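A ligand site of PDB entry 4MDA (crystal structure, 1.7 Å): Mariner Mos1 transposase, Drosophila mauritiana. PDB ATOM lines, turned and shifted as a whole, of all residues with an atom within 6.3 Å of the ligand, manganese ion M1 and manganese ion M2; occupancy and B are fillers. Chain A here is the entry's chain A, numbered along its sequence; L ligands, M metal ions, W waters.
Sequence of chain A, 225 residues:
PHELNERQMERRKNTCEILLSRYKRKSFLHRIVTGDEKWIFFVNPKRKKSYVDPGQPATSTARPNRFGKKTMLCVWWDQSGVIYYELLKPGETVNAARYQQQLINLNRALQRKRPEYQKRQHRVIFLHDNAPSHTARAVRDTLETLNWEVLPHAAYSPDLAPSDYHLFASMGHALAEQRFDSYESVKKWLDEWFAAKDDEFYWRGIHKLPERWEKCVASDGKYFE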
ATOM      1  N   PRO A   1     -10.925 -30.468   8.518  1.00  0.00           N
ATOM      2  CA  PRO A   1      -9.850 -31.111   9.273  1.00  0.00           C
ATOM      3  C   PRO A   1      -9.871 -30.745  10.766  1.00  0.00           C
ATOM      4  O   PRO A   1      -9.769 -31.623  11.637  1.00  0.00           O
ATOM      5  CB  PRO A   1      -8.583 -30.535   8.621  1.00  0.00           C
ATOM      6  CG  PRO A   1      -8.975 -29.198   8.062  1.00  0.00           C
ATOM      7  CD  PRO A   1     -10.479 -29.230   7.846  1.00  0.00           C
ATOM      8  N   HIS A   2     -10.070 -29.455  11.000  1.00  0.00           N
ATOM      9  CA  HIS A   2      -9.750 -28.745  12.229  1.00  0.00           C
ATOM     10  C   HIS A   2     -11.035 -28.438  12.992  1.00  0.00           C
ATOM     11  O   HIS A   2     -12.106 -28.330  12.390  1.00  0.00           O
ATOM     12  CB  HIS A   2      -8.999 -27.457  11.824  1.00  0.00           C
ATOM     13  CG  HIS A   2      -8.805 -26.469  12.926  1.00  0.00           C
ATOM     14  ND1 HIS A   2      -7.915 -26.666  13.957  1.00  0.00           N
ATOM     15  CD2 HIS A   2      -9.365 -25.249  13.125  1.00  0.00           C
ATOM     16  CE1 HIS A   2      -7.951 -25.622  14.762  1.00  0.00           C
ATOM     17  NE2 HIS A   2      -8.821 -24.743  14.289  1.00  0.00           N
ATOM     18  N   ARG A  11     -14.722 -14.857  12.550  1.00  0.00           N
ATOM     19  CA  ARG A  11     -13.902 -14.234  11.528  1.00  0.00           C
ATOM     20  C   ARG A  11     -14.280 -14.767  10.158  1.00  0.00           C
ATOM     21  O   ARG A  11     -14.452 -13.955   9.212  1.00  0.00           O
ATOM     22  CB  ARG A  11     -12.461 -14.394  11.858  1.00  0.00           C
ATOM     23  CG  ARG A  11     -11.528 -14.068  10.741  1.00  0.00           C
ATOM     24  CD  ARG A  11     -10.407 -13.189  11.195  1.00  0.00           C
ATOM     25  NE  ARG A  11      -9.507 -12.907  10.072  1.00  0.00           N
ATOM     26  CZ  ARG A  11      -8.265 -13.355   9.942  1.00  0.00           C
ATOM     27  NH1 ARG A  11      -7.700 -14.140  10.866  1.00  0.00           N
ATOM     28  NH2 ARG A  11      -7.565 -13.015   8.856  1.00  0.00           N
ATOM     29  N   GLY A  35      -3.253 -17.324  -5.079  1.00  0.00           N
ATOM     30  CA  GLY A  35      -2.141 -18.274  -5.100  1.00  0.00           C
ATOM     31  C   GLY A  35      -1.892 -18.870  -3.744  1.00  0.00           C
ATOM     32  O   GLY A  35      -2.408 -18.385  -2.770  1.00  0.00           O
ATOM     33  N   ASP A  36      -1.060 -19.906  -3.744  1.00  0.00           N
ATOM     34  CA  ASP A  36      -0.746 -20.609  -2.494  1.00  0.00           C
ATOM     35  C   ASP A  36       0.394 -21.584  -2.797  1.00  0.00           C
ATOM     36  O   ASP A  36       0.707 -21.858  -3.965  1.00  0.00           O
ATOM     37  CB  ASP A  36      -1.971 -21.406  -2.091  1.00  0.00           C
ATOM     38  CG  ASP A  36      -1.927 -21.942  -0.715  1.00  0.00           C
ATOM     39  OD1 ASP A  36      -1.417 -21.233   0.204  1.00  0.00           O
ATOM     40  OD2 ASP A  36      -2.514 -23.066  -0.578  1.00  0.00           O
ATOM     41  N   GLU A  37       1.035 -22.053  -1.724  1.00  0.00           N
ATOM     42  CA  GLU A  37       2.080 -23.068  -1.703  1.00  0.00           C
ATOM     43  C   GLU A  37       1.576 -24.447  -1.342  1.00  0.00           C
ATOM     44  O   GLU A  37       0.684 -24.553  -0.537  1.00  0.00           O
ATOM     45  CB  GLU A  37       3.128 -22.666  -0.684  1.00  0.00           C
ATOM     46  CG  GLU A  37       3.716 -21.273  -0.870  1.00  0.00           C
ATOM     47  CD  GLU A  37       3.012 -20.131  -0.139  1.00  0.00           C
ATOM     48  OE1 GLU A  37       3.679 -19.064   0.023  1.00  0.00           O
ATOM     49  OE2 GLU A  37       1.868 -20.293   0.350  1.00  0.00           O
ATOM     50  N   LYS A  38       2.191 -25.479  -1.948  1.00  0.00           N
ATOM     51  CA  LYS A  38       1.914 -26.878  -1.624  1.00  0.00           C
ATOM     52  C   LYS A  38       3.168 -27.708  -1.848  1.00  0.00           C
ATOM     53  O   LYS A  38       3.851 -27.551  -2.822  1.00  0.00           O
ATOM     54  CB  LYS A  38       0.801 -27.415  -2.547  1.00  0.00           C
ATOM     55  CG  LYS A  38       0.585 -28.925  -2.505  1.00  0.00           C
ATOM     56  CD  LYS A  38      -0.717 -29.314  -3.221  1.00  0.00           C
ATOM     57  CE  LYS A  38      -0.959 -30.836  -3.337  1.00  0.00           C
ATOM     58  NZ  LYS A  38      -1.243 -31.393  -1.979  1.00  0.00           N
ATOM     59  N   ASP A 129      -3.390 -16.442   1.481  1.00  0.00           N
ATOM     60  CA  ASP A 129      -3.662 -16.650   2.910  1.00  0.00           C
ATOM     61  C   ASP A 129      -2.709 -15.880   3.786  1.00  0.00           C
ATOM     62  O   ASP A 129      -1.757 -15.191   3.344  1.00  0.00           O
ATOM     63  CB  ASP A 129      -3.795 -18.159   3.186  1.00  0.00           C
ATOM     64  CG  ASP A 129      -2.537 -18.956   2.994  1.00  0.00           C
ATOM     65  OD1 ASP A 129      -1.460 -18.453   3.289  1.00  0.00           O
ATOM     66  OD2 ASP A 129      -2.628 -20.149   2.599  1.00  0.00           O
ATOM     67  N   ASN A 130      -2.958 -15.901   5.071  1.00  0.00           N
ATOM     68  CA  ASN A 130      -2.111 -15.097   5.912  1.00  0.00           C
ATOM     69  C   ASN A 130      -1.048 -15.853   6.655  1.00  0.00           C
ATOM     70  O   ASN A 130      -0.819 -15.540   7.824  1.00  0.00           O
ATOM     71  CB  ASN A 130      -2.998 -14.297   6.835  1.00  0.00           C
ATOM     72  CG  ASN A 130      -3.557 -13.081   6.138  1.00  0.00           C
ATOM     73  OD1 ASN A 130      -2.803 -12.282   5.517  1.00  0.00           O
ATOM     74  ND2 ASN A 130      -4.866 -12.997   6.118  1.00  0.00           N
ATOM     75  N   ALA A 131      -0.383 -16.805   5.985  1.00  0.00           N
ATOM     76  CA  ALA A 131       0.946 -17.308   6.408  1.00  0.00           C
ATOM     77  C   ALA A 131       1.858 -16.119   6.804  1.00  0.00           C
ATOM     78  O   ALA A 131       1.821 -15.078   6.163  1.00  0.00           O
ATOM     79  CB  ALA A 131       1.600 -18.136   5.312  1.00  0.00           C
ATOM     80  N   PRO A 132       2.700 -16.292   7.853  1.00  0.00           N
ATOM     81  CA  PRO A 132       3.557 -15.196   8.295  1.00  0.00           C
ATOM     82  C   PRO A 132       4.330 -14.527   7.159  1.00  0.00           C
ATOM     83  O   PRO A 132       4.386 -13.311   7.134  1.00  0.00           O
ATOM     84  CB  PRO A 132       4.485 -15.861   9.325  1.00  0.00           C
ATOM     85  CG  PRO A 132       3.660 -16.976   9.875  1.00  0.00           C
ATOM     86  CD  PRO A 132       2.874 -17.504   8.681  1.00  0.00           C
ATOM     87  N   HIS A 134       3.583 -14.035   4.231  1.00  0.00           N
ATOM     88  CA  HIS A 134       2.619 -13.265   3.401  1.00  0.00           C
ATOM     89  C   HIS A 134       2.233 -11.953   4.014  1.00  0.00           C
ATOM     90  O   HIS A 134       1.598 -11.099   3.335  1.00  0.00           O
ATOM     91  CB  HIS A 134       1.324 -14.107   3.187  1.00  0.00           C
ATOM     92  CG  HIS A 134       1.513 -15.351   2.390  1.00  0.00           C
ATOM     93  ND1 HIS A 134       0.454 -16.084   1.928  1.00  0.00           N
ATOM     94  CD2 HIS A 134       2.617 -15.952   1.890  1.00  0.00           C
ATOM     95  CE1 HIS A 134       0.869 -17.108   1.227  1.00  0.00           C
ATOM     96  NE2 HIS A 134       2.173 -17.049   1.176  1.00  0.00           N
ATOM     97  N   ALA A 154      -9.660 -15.445   6.231  1.00  0.00           N
ATOM     98  CA  ALA A 154      -9.634 -16.076   7.555  1.00  0.00           C
ATOM     99  C   ALA A 154      -8.718 -17.240   7.723  1.00  0.00           C
ATOM    100  O   ALA A 154      -8.551 -18.094   6.853  1.00  0.00           O
ATOM    101  CB  ALA A 154     -11.066 -16.494   7.923  1.00  0.00           C
ATOM    102  N   ALA A 155      -8.135 -17.346   8.904  1.00  0.00           N
ATOM    103  CA  ALA A 155      -7.428 -18.555   9.262  1.00  0.00           C
ATOM    104  C   ALA A 155      -8.263 -19.850   9.095  1.00  0.00           C
ATOM    105  O   ALA A 155      -9.508 -19.841   9.210  1.00  0.00           O
ATOM    106  CB  ALA A 155      -6.964 -18.425  10.714  1.00  0.00           C
ATOM    107  N   TYR A 156      -7.570 -20.929   8.838  1.00  0.00           N
ATOM    108  CA  TYR A 156      -8.145 -22.243   8.696  1.00  0.00           C
ATOM    109  C   TYR A 156      -9.266 -22.287   7.686  1.00  0.00           C
ATOM    110  O   TYR A 156     -10.280 -22.958   7.925  1.00  0.00           O
ATOM    111  CB  TYR A 156      -8.676 -22.707  10.074  1.00  0.00           C
ATOM    112  CG  TYR A 156      -7.561 -23.138  11.000  1.00  0.00           C
ATOM    113  CD1 TYR A 156      -6.960 -24.392  10.863  1.00  0.00           C
ATOM    114  CD2 TYR A 156      -7.099 -22.286  12.015  1.00  0.00           C
ATOM    115  CE1 TYR A 156      -5.920 -24.789  11.702  1.00  0.00           C
ATOM    116  CE2 TYR A 156      -6.049 -22.653  12.841  1.00  0.00           C
ATOM    117  CZ  TYR A 156      -5.471 -23.899  12.701  1.00  0.00           C
ATOM    118  OH  TYR A 156      -4.451 -24.244  13.569  1.00  0.00           O
ATOM    119  N   SER A 157      -9.094 -21.616   6.536  1.00  0.00           N
ATOM    120  CA  SER A 157     -10.171 -21.525   5.554  1.00  0.00           C
ATOM    121  C   SER A 157      -9.716 -21.917   4.149  1.00  0.00           C
ATOM    122  O   SER A 157      -9.920 -21.182   3.245  1.00  0.00           O
ATOM    123  CB  SER A 157     -10.758 -20.151   5.568  1.00  0.00           C
ATOM    124  OG  SER A 157     -11.245 -19.773   6.885  1.00  0.00           O
ATOM    125  N   PRO A 158      -9.197 -23.142   3.982  1.00  0.00           N
ATOM    126  CA  PRO A 158      -8.843 -23.614   2.617  1.00  0.00           C
ATOM    127  C   PRO A 158     -10.115 -23.862   1.794  1.00  0.00           C
ATOM    128  O   PRO A 158     -10.088 -23.905   0.537  1.00  0.00           O
ATOM    129  CB  PRO A 158      -8.045 -24.897   2.919  1.00  0.00           C
ATOM    130  CG  PRO A 158      -8.790 -25.433   4.143  1.00  0.00           C
ATOM    131  CD  PRO A 158      -8.915 -24.203   4.972  1.00  0.00           C
ATOM    132  N   ALA A 161     -10.343 -20.682  -0.155  1.00  0.00           N
ATOM    133  CA  ALA A 161      -9.136 -20.389  -0.978  1.00  0.00           C
ATOM    134  C   ALA A 161      -9.184 -21.216  -2.262  1.00  0.00           C
ATOM    135  O   ALA A 161      -9.055 -22.454  -2.205  1.00  0.00           O
ATOM    136  CB  ALA A 161      -7.866 -20.756  -0.192  1.00  0.00           C
ATOM    137  N   SER A 163      -7.131 -21.899  -4.573  1.00  0.00           N
ATOM    138  CA  SER A 163      -6.014 -22.788  -4.768  1.00  0.00           C
ATOM    139  C   SER A 163      -6.218 -24.146  -4.074  1.00  0.00           C
ATOM    140  O   SER A 163      -5.783 -25.166  -4.597  1.00  0.00           O
ATOM    141  CB  SER A 163      -4.678 -22.151  -4.354  1.00  0.00           C
ATOM    142  OG  SER A 163      -4.417 -20.928  -5.025  1.00  0.00           O
ATOM    143  N   ASP A 164      -6.828 -24.072  -2.889  1.00  0.00           N
ATOM    144  CA  ASP A 164      -7.040 -25.278  -2.093  1.00  0.00           C
ATOM    145  C   ASP A 164      -8.289 -26.027  -2.547  1.00  0.00           C
ATOM    146  O   ASP A 164      -8.184 -27.225  -2.887  1.00  0.00           O
ATOM    147  CB  ASP A 164      -7.032 -24.930  -0.606  1.00  0.00           C
ATOM    148  CG  ASP A 164      -5.637 -24.614  -0.094  1.00  0.00           C
ATOM    149  OD1 ASP A 164      -4.691 -25.384  -0.409  1.00  0.00           O
ATOM    150  OD2 ASP A 164      -5.433 -23.609   0.644  1.00  0.00           O
ATOM    151  N   PHE A 168      -5.576 -27.337  -6.183  1.00  0.00           N
ATOM    152  CA  PHE A 168      -4.844 -28.415  -5.502  1.00  0.00           C
ATOM    153  C   PHE A 168      -5.713 -29.632  -5.210  1.00  0.00           C
ATOM    154  O   PHE A 168      -5.204 -30.698  -5.139  1.00  0.00           O
ATOM    155  CB  PHE A 168      -4.207 -27.961  -4.203  1.00  0.00           C
ATOM    156  CG  PHE A 168      -3.151 -26.859  -4.337  1.00  0.00           C
ATOM    157  CD1 PHE A 168      -2.347 -26.750  -5.480  1.00  0.00           C
ATOM    158  CD2 PHE A 168      -2.881 -25.992  -3.273  1.00  0.00           C
ATOM    159  CE1 PHE A 168      -1.403 -25.727  -5.582  1.00  0.00           C
ATOM    160  CE2 PHE A 168      -1.901 -24.996  -3.378  1.00  0.00           C
ATOM    161  CZ  PHE A 168      -1.131 -24.891  -4.558  1.00  0.00           C
ATOM    162  N   TYR A 223     -17.421 -24.926   8.936  1.00  0.00           N
ATOM    163  CA  TYR A 223     -17.221 -25.624   7.689  1.00  0.00           C
ATOM    164  C   TYR A 223     -18.550 -26.110   7.200  1.00  0.00           C
ATOM    165  O   TYR A 223     -19.529 -26.189   7.983  1.00  0.00           O
ATOM    166  CB  TYR A 223     -16.257 -26.823   7.874  1.00  0.00           C
ATOM    167  CG  TYR A 223     -14.864 -26.424   8.271  1.00  0.00           C
ATOM    168  CD1 TYR A 223     -14.156 -25.478   7.513  1.00  0.00           C
ATOM    169  CD2 TYR A 223     -14.244 -26.962   9.382  1.00  0.00           C
ATOM    170  CE1 TYR A 223     -12.851 -25.151   7.824  1.00  0.00           C
ATOM    171  CE2 TYR A 223     -12.960 -26.578   9.736  1.00  0.00           C
ATOM    172  CZ  TYR A 223     -12.266 -25.680   8.960  1.00  0.00           C
ATOM    173  OH  TYR A 223     -11.039 -25.338   9.354  1.00  0.00           O
HETATM  174  C1  LIG L   1      -4.431 -19.896  10.385  1.00  0.00           C
HETATM  175  C2  LIG L   1      -4.782 -27.103   4.325  1.00  0.00           C
HETATM  176  C3  LIG L   1      -5.255 -26.687   7.288  1.00  0.00           C
HETATM  177  C4  LIG L   1      -2.704 -27.287   7.418  1.00  0.00           C
HETATM  178  O1  LIG L   1      -0.945 -21.965   4.466  1.00  0.00           O
HETATM  179  O2  LIG L   1      -5.304 -23.655   7.678  1.00  0.00           O
HETATM  180  O3  LIG L   1      -4.018 -25.763   2.505  1.00  0.00           O
HETATM  181  O4  LIG L   1      -2.502 -23.470   2.548  1.00  0.00           O
HETATM  182  F1  LIG L   1      -2.804 -17.689  10.161  1.00  0.00           F
HETATM  183  C5  LIG L   1      -2.284 -18.684   8.097  1.00  0.00           C
HETATM  184  C6  LIG L   1      -1.331 -19.571  10.085  1.00  0.00           C
HETATM  185  C7  LIG L   1      -1.589 -19.633   7.349  1.00  0.00           C
HETATM  186  C8  LIG L   1      -0.664 -20.545   9.363  1.00  0.00           C
HETATM  187  C9  LIG L   1      -0.076 -21.615   7.165  1.00  0.00           C
HETATM  188  N1  LIG L   1      -2.943 -21.986  11.075  1.00  0.00           N
HETATM  189  N2  LIG L   1      -2.918 -23.249  10.443  1.00  0.00           N
HETATM  190  N3  LIG L   1      -2.710 -24.419   6.148  1.00  0.00           N
HETATM  191  N4  LIG L   1      -1.070 -22.609   6.650  1.00  0.00           N
HETATM  192  N5  LIG L   1      -3.575 -25.164   8.289  1.00  0.00           N
HETATM  193  O5  LIG L   1      -4.424 -21.909   9.373  1.00  0.00           O
HETATM  194  C10 LIG L   1      -1.408 -22.629   5.355  1.00  0.00           C
HETATM  195  C11 LIG L   1      -4.315 -24.025   8.371  1.00  0.00           C
HETATM  196  C12 LIG L   1      -3.833 -21.247  10.369  1.00  0.00           C
HETATM  197  C13 LIG L   1      -2.127 -18.630   9.463  1.00  0.00           C
HETATM  198  C14 LIG L   1      -0.787 -20.581   7.975  1.00  0.00           C
HETATM  199  C15 LIG L   1      -2.748 -24.054   3.719  1.00  0.00           C
HETATM  200  C16 LIG L   1      -3.822 -23.126   9.429  1.00  0.00           C
HETATM  201  C17 LIG L   1      -2.285 -23.719   5.049  1.00  0.00           C
HETATM  202  C18 LIG L   1      -3.497 -25.532   6.103  1.00  0.00           C
HETATM  203  C19 LIG L   1      -3.595 -25.243   3.620  1.00  0.00           C
HETATM  204  N6  LIG L   1      -3.910 -25.936   4.775  1.00  0.00           N
HETATM  205  C20 LIG L   1      -3.819 -26.300   7.492  1.00  0.00           C
HETATM  206 MN    MN M   1      -1.140 -21.809   2.317  1.00  0.00          MN
HETATM  207 MN    MN M   2      -3.194 -24.492   0.818  1.00  0.00          MN
HETATM  208  O   HOH W   1      -1.622 -25.848   0.266  1.00  0.00           O
HETATM  209  O   HOH W   2       0.416 -20.335   2.523  1.00  0.00           O
HETATM  210  O   HOH W   3      -0.376 -24.718   9.100  1.00  0.00           O
HETATM  211  O   HOH W   4      -1.409 -27.862   4.421  1.00  0.00           O
HETATM  212  O   HOH W   5       0.425 -23.288   1.842  1.00  0.00           O
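Manganese ion M2 is bound by OD2 of Asp 36 (2.1 Å), O4 of the ligand (2.1 Å), OD1 of Asp 164 (2.1 Å), water W1 (2.1 Å), O3 of the ligand (2.3 Å) and OD2 of Asp 164 (2.4 Å).
N of Tyr 156 lies within hydrogen-bond range of O5 of the ligand, at 3.3 Å.
Asn 130 touches the ligand. Ala 131 touches the ligand (N to C7, 3.4 Å). Ala 155 touches the ligand (CB to C1, 2.9 Å). Within 4 Å of the ligand: Asp 36, Asp 129, Asn 130, Ala 131, Ala 155, Tyr 156 and Asp 164. Along chain A the residues within 4 Å of the ligand span positions 36 to 164. The nearest printed residue that does not touch the ligand is Pro 158 (4.1 Å).
Manganese ion M1 is bound by water W2, an oxygen (O4) of the ligand, an oxygen (O1) of the ligand, water W5, the side-chain carboxylate (OD1) of Asp 36 and the side-chain carboxylate (OD2) of Asp 129.
Water W2 bridges OE2 of Glu 37 and OD1 of Asp 129.
Merely in contact with manganese ion M1: Glu 37 (3.9 Å). Along chain A the residues within 4 Å of manganese ion M1 span positions 36 to 129. The nearest printed residue that does not touch manganese ion M1 is Asp 164 (4.9 Å).
The side-chain carboxylate (OD1) of Asp 129 sits close to the backbone NH (N) of Ala 131, 3.3 Å away. The backbone carbonyl oxygen (O) of Ala 155 lies within hydrogen-bond range of the side-chain hydroxyl (OG) of Ser 157 (2.9 Å). O of Asp 129 lies within hydrogen-bond range of ND1 of His 134 (2.8 Å). The side-chain carboxylate (OE1) of Glu 37 is in hydrogen-bond range of a ring nitrogen (NE2) of His 134. OH of Tyr 223 lies within hydrogen-bond range of O of Tyr 156, at 2.9 Å.
Two residues have an atom within 4 Å of manganese ion M2: Asp 36 and Asp 164. The nearest printed residue that does not touch manganese ion M2 is Glu 37 (4.1 Å).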
